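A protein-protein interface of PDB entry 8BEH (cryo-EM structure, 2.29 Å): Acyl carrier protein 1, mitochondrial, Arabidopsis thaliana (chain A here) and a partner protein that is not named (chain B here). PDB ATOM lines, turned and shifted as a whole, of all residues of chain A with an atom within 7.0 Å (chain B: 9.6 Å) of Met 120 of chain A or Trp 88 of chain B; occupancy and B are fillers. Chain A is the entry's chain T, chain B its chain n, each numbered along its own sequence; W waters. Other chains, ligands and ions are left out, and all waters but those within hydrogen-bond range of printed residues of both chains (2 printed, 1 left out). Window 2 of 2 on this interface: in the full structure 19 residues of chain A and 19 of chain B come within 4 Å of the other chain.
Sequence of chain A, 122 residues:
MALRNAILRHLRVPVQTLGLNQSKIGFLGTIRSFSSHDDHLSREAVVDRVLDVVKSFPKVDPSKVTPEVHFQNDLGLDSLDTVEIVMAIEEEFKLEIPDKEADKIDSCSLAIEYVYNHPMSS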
ATOM      1  N   HIS A  40     -42.133  13.316  -3.013  1.00  0.00           N
ATOM      2  CA  HIS A  40     -41.095  13.873  -2.092  1.00  0.00           C
ATOM      3  C   HIS A  40     -40.597  12.787  -1.172  1.00  0.00           C
ATOM      4  O   HIS A  40     -41.203  11.695  -1.149  1.00  0.00           O
ATOM      5  CB  HIS A  40     -41.649  15.057  -1.308  1.00  0.00           C
ATOM      6  CG  HIS A  40     -42.097  16.169  -2.194  1.00  0.00           C
ATOM      7  ND1 HIS A  40     -41.205  16.930  -2.921  1.00  0.00           N
ATOM      8  CD2 HIS A  40     -43.325  16.664  -2.457  1.00  0.00           C
ATOM      9  CE1 HIS A  40     -41.867  17.838  -3.608  1.00  0.00           C
ATOM     10  NE2 HIS A  40     -43.169  17.697  -3.338  1.00  0.00           N
ATOM     11  N   GLU A  90     -24.131  14.256  -0.763  1.00  0.00           N
ATOM     12  CA  GLU A  90     -24.381  14.695  -2.132  1.00  0.00           C
ATOM     13  C   GLU A  90     -24.595  13.506  -3.058  1.00  0.00           C
ATOM     14  O   GLU A  90     -25.562  13.462  -3.823  1.00  0.00           O
ATOM     15  CB  GLU A  90     -23.197  15.529  -2.626  1.00  0.00           C
ATOM     16  CG  GLU A  90     -23.172  16.976  -2.186  1.00  0.00           C
ATOM     17  CD  GLU A  90     -24.023  17.850  -3.068  1.00  0.00           C
ATOM     18  OE1 GLU A  90     -25.255  17.684  -3.039  1.00  0.00           O
ATOM     19  OE2 GLU A  90     -23.466  18.704  -3.789  1.00  0.00           O
ATOM     20  N   PHE A  93     -27.992  11.432  -2.307  1.00  0.00           N
ATOM     21  CA  PHE A  93     -29.318  11.943  -2.740  1.00  0.00           C
ATOM     22  C   PHE A  93     -29.242  12.474  -4.184  1.00  0.00           C
ATOM     23  O   PHE A  93     -30.275  12.956  -4.625  1.00  0.00           O
ATOM     24  CB  PHE A  93     -29.888  12.975  -1.730  1.00  0.00           C
ATOM     25  CG  PHE A  93     -30.295  12.412  -0.394  1.00  0.00           C
ATOM     26  CD1 PHE A  93     -31.552  11.864  -0.208  1.00  0.00           C
ATOM     27  CD2 PHE A  93     -29.424  12.430   0.681  1.00  0.00           C
ATOM     28  CE1 PHE A  93     -31.931  11.356   1.022  1.00  0.00           C
ATOM     29  CE2 PHE A  93     -29.798  11.912   1.908  1.00  0.00           C
ATOM     30  CZ  PHE A  93     -31.053  11.378   2.076  1.00  0.00           C
ATOM     31  N   LYS A  94     -28.079  12.385  -4.881  1.00  0.00           N
ATOM     32  CA  LYS A  94     -27.907  12.979  -6.248  1.00  0.00           C
ATOM     33  C   LYS A  94     -28.202  14.492  -6.213  1.00  0.00           C
ATOM     34  O   LYS A  94     -28.984  14.953  -7.004  1.00  0.00           O
ATOM     35  CB  LYS A  94     -28.565  12.209  -7.411  1.00  0.00           C
ATOM     36  CG  LYS A  94     -27.900  12.446  -8.754  1.00  0.00           C
ATOM     37  CD  LYS A  94     -28.630  11.962  -9.982  1.00  0.00           C
ATOM     38  CE  LYS A  94     -27.835  12.279 -11.237  1.00  0.00           C
ATOM     39  NZ  LYS A  94     -28.468  11.793 -12.483  1.00  0.00           N
ATOM     40  N   LEU A  95     -27.439  15.237  -5.438  1.00  0.00           N
ATOM     41  CA  LEU A  95     -27.610  16.681  -5.435  1.00  0.00           C
ATOM     42  C   LEU A  95     -26.291  17.348  -5.790  1.00  0.00           C
ATOM     43  O   LEU A  95     -25.218  16.750  -5.688  1.00  0.00           O
ATOM     44  CB  LEU A  95     -28.111  17.200  -4.082  1.00  0.00           C
ATOM     45  CG  LEU A  95     -29.246  16.434  -3.408  1.00  0.00           C
ATOM     46  CD1 LEU A  95     -29.321  16.772  -1.925  1.00  0.00           C
ATOM     47  CD2 LEU A  95     -30.567  16.684  -4.105  1.00  0.00           C
ATOM     48  N   GLU A  96     -26.383  18.596  -6.229  1.00  0.00           N
ATOM     49  CA  GLU A  96     -25.211  19.426  -6.499  1.00  0.00           C
ATOM     50  C   GLU A  96     -25.346  20.676  -5.638  1.00  0.00           C
ATOM     51  O   GLU A  96     -25.943  21.669  -6.064  1.00  0.00           O
ATOM     52  CB  GLU A  96     -25.090  19.765  -7.982  1.00  0.00           C
ATOM     53  CG  GLU A  96     -23.747  20.362  -8.367  1.00  0.00           C
ATOM     54  CD  GLU A  96     -23.286  19.945  -9.758  1.00  0.00           C
ATOM     55  OE1 GLU A  96     -23.399  18.752 -10.091  1.00  0.00           O
ATOM     56  OE2 GLU A  96     -22.797  20.808 -10.513  1.00  0.00           O
ATOM     57  N   ILE A  97     -24.811  20.618  -4.429  1.00  0.00           N
ATOM     58  CA  ILE A  97     -24.872  21.759  -3.513  1.00  0.00           C
ATOM     59  C   ILE A  97     -23.837  22.794  -3.945  1.00  0.00           C
ATOM     60  O   ILE A  97     -22.690  22.427  -4.237  1.00  0.00           O
ATOM     61  CB  ILE A  97     -24.632  21.307  -2.078  1.00  0.00           C
ATOM     62  CG1 ILE A  97     -25.743  20.362  -1.636  1.00  0.00           C
ATOM     63  CG2 ILE A  97     -24.578  22.507  -1.143  1.00  0.00           C
ATOM     64  CD1 ILE A  97     -25.424  19.562  -0.402  1.00  0.00           C
ATOM     65  N   VAL A 115     -31.314  18.631   2.858  1.00  0.00           N
ATOM     66  CA  VAL A 115     -31.792  17.580   1.964  1.00  0.00           C
ATOM     67  C   VAL A 115     -33.315  17.542   1.944  1.00  0.00           C
ATOM     68  O   VAL A 115     -33.930  17.413   0.879  1.00  0.00           O
ATOM     69  CB  VAL A 115     -31.186  16.221   2.359  1.00  0.00           C
ATOM     70  CG1 VAL A 115     -31.840  15.088   1.580  1.00  0.00           C
ATOM     71  CG2 VAL A 115     -29.686  16.230   2.113  1.00  0.00           C
ATOM     72  N   ASN A 117     -35.416  20.011   2.547  1.00  0.00           N
ATOM     73  CA  ASN A 117     -35.978  21.183   1.892  1.00  0.00           C
ATOM     74  C   ASN A 117     -35.657  21.248   0.408  1.00  0.00           C
ATOM     75  O   ASN A 117     -36.312  22.003  -0.317  1.00  0.00           O
ATOM     76  CB  ASN A 117     -35.485  22.454   2.579  1.00  0.00           C
ATOM     77  CG  ASN A 117     -35.852  22.495   4.040  1.00  0.00           C
ATOM     78  OD1 ASN A 117     -35.124  23.051   4.857  1.00  0.00           O
ATOM     79  ND2 ASN A 117     -36.975  21.883   4.382  1.00  0.00           N
ATOM     80  N   HIS A 118     -34.675  20.495  -0.064  1.00  0.00           N
ATOM     81  CA  HIS A 118     -34.367  20.528  -1.484  1.00  0.00           C
ATOM     82  C   HIS A 118     -35.463  19.800  -2.254  1.00  0.00           C
ATOM     83  O   HIS A 118     -35.758  18.639  -1.955  1.00  0.00           O
ATOM     84  CB  HIS A 118     -33.010  19.904  -1.786  1.00  0.00           C
ATOM     85  CG  HIS A 118     -32.401  20.405  -3.057  1.00  0.00           C
ATOM     86  ND1 HIS A 118     -32.734  21.623  -3.603  1.00  0.00           N
ATOM     87  CD2 HIS A 118     -31.525  19.838  -3.915  1.00  0.00           C
ATOM     88  CE1 HIS A 118     -32.068  21.798  -4.730  1.00  0.00           C
ATOM     89  NE2 HIS A 118     -31.329  20.726  -4.943  1.00  0.00           N
ATOM     90  N   PRO A 119     -36.100  20.449  -3.230  1.00  0.00           N
ATOM     91  CA  PRO A 119     -37.182  19.782  -3.969  1.00  0.00           C
ATOM     92  C   PRO A 119     -36.720  18.659  -4.877  1.00  0.00           C
ATOM     93  O   PRO A 119     -37.543  17.812  -5.244  1.00  0.00           O
ATOM     94  CB  PRO A 119     -37.798  20.924  -4.787  1.00  0.00           C
ATOM     95  CG  PRO A 119     -36.705  21.899  -4.942  1.00  0.00           C
ATOM     96  CD  PRO A 119     -35.881  21.827  -3.696  1.00  0.00           C
ATOM     97  N   MET A 120     -35.451  18.617  -5.259  1.00  0.00           N
ATOM     98  CA  MET A 120     -34.982  17.595  -6.180  1.00  0.00           C
ATOM     99  C   MET A 120     -34.334  16.415  -5.473  1.00  0.00           C
ATOM    100  O   MET A 120     -33.783  15.538  -6.143  1.00  0.00           O
ATOM    101  CB  MET A 120     -34.007  18.196  -7.190  1.00  0.00           C
ATOM    102  CG  MET A 120     -34.684  19.019  -8.266  1.00  0.00           C
ATOM    103  SD  MET A 120     -35.473  18.030  -9.545  1.00  0.00           S
ATOM    104  CE  MET A 120     -34.398  16.608  -9.636  1.00  0.00           C
ATOM    105  N   SER A 121     -34.397  16.321  -4.149  1.00  0.00           N
ATOM    106  CA  SER A 121     -33.818  15.147  -3.433  1.00  0.00           C
ATOM    107  C   SER A 121     -34.631  13.864  -3.664  1.00  0.00           C
ATOM    108  O   SER A 121     -34.029  12.780  -3.681  1.00  0.00           O
ATOM    109  CB  SER A 121     -33.670  15.441  -1.971  1.00  0.00           C
ATOM    110  OG  SER A 121     -32.955  16.648  -1.761  1.00  0.00           O
ATOM    111  N   TYR B  84     -18.179  16.764 -14.601  1.00  0.00           N
ATOM    112  CA  TYR B  84     -19.531  16.241 -14.494  1.00  0.00           C
ATOM    113  C   TYR B  84     -20.433  17.234 -13.773  1.00  0.00           C
ATOM    114  O   TYR B  84     -20.038  17.849 -12.780  1.00  0.00           O
ATOM    115  CB  TYR B  84     -19.542  14.908 -13.743  1.00  0.00           C
ATOM    116  CG  TYR B  84     -20.942  14.474 -13.396  1.00  0.00           C
ATOM    117  CD1 TYR B  84     -21.768  13.907 -14.358  1.00  0.00           C
ATOM    118  CD2 TYR B  84     -21.463  14.686 -12.126  1.00  0.00           C
ATOM    119  CE1 TYR B  84     -23.057  13.540 -14.058  1.00  0.00           C
ATOM    120  CE2 TYR B  84     -22.755  14.324 -11.819  1.00  0.00           C
ATOM    121  CZ  TYR B  84     -23.548  13.750 -12.787  1.00  0.00           C
ATOM    122  OH  TYR B  84     -24.832  13.381 -12.484  1.00  0.00           O
ATOM    123  N   ILE B  85     -21.656  17.380 -14.266  1.00  0.00           N
ATOM    124  CA  ILE B  85     -22.670  18.200 -13.616  1.00  0.00           C
ATOM    125  C   ILE B  85     -23.972  17.416 -13.570  1.00  0.00           C
ATOM    126  O   ILE B  85     -24.370  16.804 -14.565  1.00  0.00           O
ATOM    127  CB  ILE B  85     -22.879  19.554 -14.333  1.00  0.00           C
ATOM    128  CG1 ILE B  85     -21.567  20.328 -14.444  1.00  0.00           C
ATOM    129  CG2 ILE B  85     -23.931  20.394 -13.614  1.00  0.00           C
ATOM    130  CD1 ILE B  85     -21.359  20.990 -15.780  1.00  0.00           C
ATOM    131  N   VAL B  86     -24.631  17.439 -12.416  1.00  0.00           N
ATOM    132  CA  VAL B  86     -25.985  16.883 -12.312  1.00  0.00           C
ATOM    133  C   VAL B  86     -26.882  17.568 -13.338  1.00  0.00           C
ATOM    134  O   VAL B  86     -26.828  18.805 -13.479  1.00  0.00           O
ATOM    135  CB  VAL B  86     -26.529  17.068 -10.883  1.00  0.00           C
ATOM    136  CG1 VAL B  86     -27.900  16.439 -10.729  1.00  0.00           C
ATOM    137  CG2 VAL B  86     -25.560  16.477  -9.870  1.00  0.00           C
ATOM    138  N   PRO B  87     -27.705  16.824 -14.085  1.00  0.00           N
ATOM    139  CA  PRO B  87     -28.388  17.422 -15.249  1.00  0.00           C
ATOM    140  C   PRO B  87     -29.258  18.631 -14.935  1.00  0.00           C
ATOM    141  O   PRO B  87     -29.368  19.525 -15.781  1.00  0.00           O
ATOM    142  CB  PRO B  87     -29.218  16.252 -15.795  1.00  0.00           C
ATOM    143  CG  PRO B  87     -28.503  15.042 -15.342  1.00  0.00           C
ATOM    144  CD  PRO B  87     -27.919  15.369 -14.006  1.00  0.00           C
ATOM    145  N   TRP B  88     -29.879  18.696 -13.760  1.00  0.00           N
ATOM    146  CA  TRP B  88     -30.736  19.829 -13.429  1.00  0.00           C
ATOM    147  C   TRP B  88     -29.993  20.973 -12.744  1.00  0.00           C
ATOM    148  O   TRP B  88     -30.595  22.021 -12.503  1.00  0.00           O
ATOM    149  CB  TRP B  88     -31.912  19.376 -12.556  1.00  0.00           C
ATOM    150  CG  TRP B  88     -31.539  18.499 -11.414  1.00  0.00           C
ATOM    151  CD1 TRP B  88     -31.647  17.142 -11.357  1.00  0.00           C
ATOM    152  CD2 TRP B  88     -30.994  18.910 -10.157  1.00  0.00           C
ATOM    153  NE1 TRP B  88     -31.206  16.682 -10.144  1.00  0.00           N
ATOM    154  CE2 TRP B  88     -30.797  17.747  -9.388  1.00  0.00           C
ATOM    155  CE3 TRP B  88     -30.647  20.148  -9.609  1.00  0.00           C
ATOM    156  CZ2 TRP B  88     -30.272  17.786  -8.099  1.00  0.00           C
ATOM    157  CZ3 TRP B  88     -30.125  20.183  -8.330  1.00  0.00           C
ATOM    158  CH2 TRP B  88     -29.942  19.011  -7.591  1.00  0.00           C
ATOM    159  N   ALA B  89     -28.716  20.803 -12.429  1.00  0.00           N
ATOM    160  CA  ALA B  89     -27.917  21.865 -11.841  1.00  0.00           C
ATOM    161  C   ALA B  89     -27.514  22.882 -12.906  1.00  0.00           C
ATOM    162  O   ALA B  89     -27.572  22.592 -14.103  1.00  0.00           O
ATOM    163  CB  ALA B  89     -26.686  21.272 -11.166  1.00  0.00           C
ATOM    164  N   PRO B  90     -27.137  24.096 -12.502  1.00  0.00           N
ATOM    165  CA  PRO B  90     -26.704  25.094 -13.490  1.00  0.00           C
ATOM    166  C   PRO B  90     -25.534  24.586 -14.321  1.00  0.00           C
ATOM    167  O   PRO B  90     -24.543  24.082 -13.792  1.00  0.00           O
ATOM    168  CB  PRO B  90     -26.310  26.303 -12.630  1.00  0.00           C
ATOM    169  CG  PRO B  90     -26.260  25.808 -11.232  1.00  0.00           C
ATOM    170  CD  PRO B  90     -27.200  24.665 -11.146  1.00  0.00           C
ATOM    171  N   GLY B  91     -25.659  24.735 -15.638  1.00  0.00           N
ATOM    172  CA  GLY B  91     -24.731  24.136 -16.569  1.00  0.00           C
ATOM    173  C   GLY B  91     -25.070  22.717 -16.970  1.00  0.00           C
ATOM    174  O   GLY B  91     -24.416  22.172 -17.866  1.00  0.00           O
ATOM    175  N   GLY B  92     -26.080  22.106 -16.347  1.00  0.00           N
ATOM    176  CA  GLY B  92     -26.442  20.742 -16.654  1.00  0.00           C
ATOM    177  C   GLY B  92     -27.235  20.610 -17.939  1.00  0.00           C
ATOM    178  O   GLY B  92     -27.731  21.578 -18.510  1.00  0.00           O
ATOM    179  N   SER B  93     -27.362  19.361 -18.391  1.00  0.00           N
ATOM    180  CA  SER B  93     -28.048  19.092 -19.648  1.00  0.00           C
ATOM    181  C   SER B  93     -29.551  19.329 -19.558  1.00  0.00           C
ATOM    182  O   SER B  93     -30.177  19.625 -20.579  1.00  0.00           O
ATOM    183  CB  SER B  93     -27.757  17.659 -20.101  1.00  0.00           C
ATOM    184  OG  SER B  93     -28.320  16.714 -19.210  1.00  0.00           O
ATOM    185  N   LYS B  94     -30.138  19.218 -18.368  1.00  0.00           N
ATOM    186  CA  LYS B  94     -31.562  19.448 -18.151  1.00  0.00           C
ATOM    187  C   LYS B  94     -31.876  20.824 -17.569  1.00  0.00           C
ATOM    188  O   LYS B  94     -33.042  21.109 -17.283  1.00  0.00           O
ATOM    189  CB  LYS B  94     -32.138  18.371 -17.233  1.00  0.00           C
ATOM    190  CG  LYS B  94     -33.363  17.683 -17.775  1.00  0.00           C
ATOM    191  CD  LYS B  94     -34.217  17.155 -16.645  1.00  0.00           C
ATOM    192  CE  LYS B  94     -35.317  16.258 -17.152  1.00  0.00           C
ATOM    193  NZ  LYS B  94     -35.891  15.427 -16.064  1.00  0.00           N
ATOM    194  N   PHE B  95     -30.874  21.678 -17.384  1.00  0.00           N
ATOM    195  CA  PHE B  95     -31.079  22.946 -16.696  1.00  0.00           C
ATOM    196  C   PHE B  95     -31.958  23.878 -17.526  1.00  0.00           C
ATOM    197  O   PHE B  95     -31.692  24.111 -18.709  1.00  0.00           O
ATOM    198  CB  PHE B  95     -29.728  23.596 -16.396  1.00  0.00           C
ATOM    199  CG  PHE B  95     -29.810  24.784 -15.478  1.00  0.00           C
ATOM    200  CD1 PHE B  95     -30.480  24.700 -14.268  1.00  0.00           C
ATOM    201  CD2 PHE B  95     -29.204  25.982 -15.819  1.00  0.00           C
ATOM    202  CE1 PHE B  95     -30.556  25.794 -13.419  1.00  0.00           C
ATOM    203  CE2 PHE B  95     -29.277  27.080 -14.971  1.00  0.00           C
ATOM    204  CZ  PHE B  95     -29.954  26.983 -13.772  1.00  0.00           C
ATOM    205  N   CYS B  96     -33.014  24.404 -16.897  1.00  0.00           N
ATOM    206  CA  CYS B  96     -33.955  25.354 -17.504  1.00  0.00           C
ATOM    207  C   CYS B  96     -34.764  24.745 -18.652  1.00  0.00           C
ATOM    208  O   CYS B  96     -35.184  25.463 -19.560  1.00  0.00           O
ATOM    209  CB  CYS B  96     -33.241  26.620 -17.991  1.00  0.00           C
ATOM    210  SG  CYS B  96     -32.165  27.423 -16.783  1.00  0.00           S
ATOM    211  N   ARG B  97     -34.950  23.433 -18.563  1.00  0.00           N
ATOM    212  CA  ARG B  97     -35.886  22.738 -19.429  1.00  0.00           C
ATOM    213  C   ARG B  97     -37.229  22.653 -18.705  1.00  0.00           C
ATOM    214  O   ARG B  97     -37.226  22.297 -17.578  1.00  0.00           O
ATOM    215  CB  ARG B  97     -35.421  21.317 -19.728  1.00  0.00           C
ATOM    216  CG  ARG B  97     -36.261  20.620 -20.788  1.00  0.00           C
ATOM    217  CD  ARG B  97     -36.088  19.117 -20.823  1.00  0.00           C
ATOM    218  NE  ARG B  97     -34.789  18.742 -21.342  1.00  0.00           N
ATOM    219  CZ  ARG B  97     -34.295  17.513 -21.373  1.00  0.00           C
ATOM    220  NH1 ARG B  97     -34.997  16.499 -20.901  1.00  0.00           N
ATOM    221  NH2 ARG B  97     -33.099  17.307 -21.880  1.00  0.00           N
HETATM  222  O   HOH W   1     -24.068  23.338 -11.395  1.00  0.00           O
HETATM  223  O   HOH W   2     -20.625  20.149 -11.470  1.00  0.00           O
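N of Ser 93 of chain B is in hydrogen-bond range of O of Pro 87 of chain B (3.3 Å).
The backbone NH (N) of Phe 95 of chain B sits at hydrogen-bond distance from the backbone carbonyl oxygen (O) of Pro 87 of chain B (3.1 Å).
O of Glu 90 of chain A is in hydrogen-bond range of N of Leu 95 of chain A (3.0 Å).
O of Pro 87 of chain B is in hydrogen-bond range of N of Lys 94 of chain B, at 2.7 Å.
The backbone carbonyl oxygen (O) of His 118 of chain A lies close to the side-chain hydroxyl (OG) of Ser 121 of chain A (3.4 Å).
N of Val 86 of chain B lies within hydrogen-bond range of OE1 of Glu 96 of chain A (2.9 Å).
Glu 90 of chain A touches none of the printed residues of chain B.
Printed residues of chain B within 4 Å of Glu 96 of chain A: Ile 85, Val 86, Trp 88 and Ala 89.
Printed residues of chain B within 4 Å of His 118 of chain A: Trp 88 (3.4 Å).
No residue of chain B comes within 4 Å of Ser 121 of chain A.
Printed residues of chain A within 4 Å of Tyr 84 of chain B: Lys 94 (3.4 Å).
Trp 88 of chain B touches just these residues of chain A: Lys 94, Leu 95, Glu 96, His 118 and Met 120.
Lys 94 of chain B touches none of the printed residues of chain A.
The nearest residue of chain B that does not touch Met 120 of chain A is Val 86 of chain B (6.6 Å).
The nearest residue of chain A that does not touch Trp 88 of chain B is Ser 121 of chain A (5.9 Å).
Among the printed residues, pairs that only touch across the chains: Lys 94 of chain A with Tyr 84 of chain B (3.4 Å), Lys 94 of chain A with Pro 87 of chain B (3.9 Å), Lys 94 of chain A with Trp 88 of chain B (3.3 Å), Leu 95 of chain A with Trp 88 of chain B (3.9 Å), Glu 96 of chain A with Ile 85 of chain B (3.3 Å), Glu 96 of chain A with Trp 88 of chain B (3.8 Å), Glu 96 of chain A with Ala 89 of chain B (3.9 Å), His 118 of chain A with Trp 88 of chain B (3.4 Å) and Met 120 of chain A with Trp 88 of chain B (3.2 Å).
Of the 13 printed residues of chain A, 5 touch a printed residue of chain B.
Printed residues of chain A that touch a printed residue of chain B: Lys 94, Leu 95, Glu 96, His 118 and Met 120.
Hydrophobic or aromatic side chains of chain A that line the printed part of chain B: His 118 and Met 120.
Of the 14 printed residues of chain B, 6 touch a printed residue of chain A.
Among the printed residues, 10 pairs touch across the chains.
Among the printed residues, no Asp or Glu carboxylate lies within 4 Å of a Lys or Arg side-chain nitrogen of the other chain.
Water W2 lies within hydrogen-bond range of OE2 of Glu 96 of chain A (2.5 Å) and O of Tyr 84 of chain B (2.7 Å).
Water W1 bridges the backbone carbonyl oxygen (O) of Pro 90 of chain B and the side-chain carboxylate (OE2) of Glu 96 of chain A.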
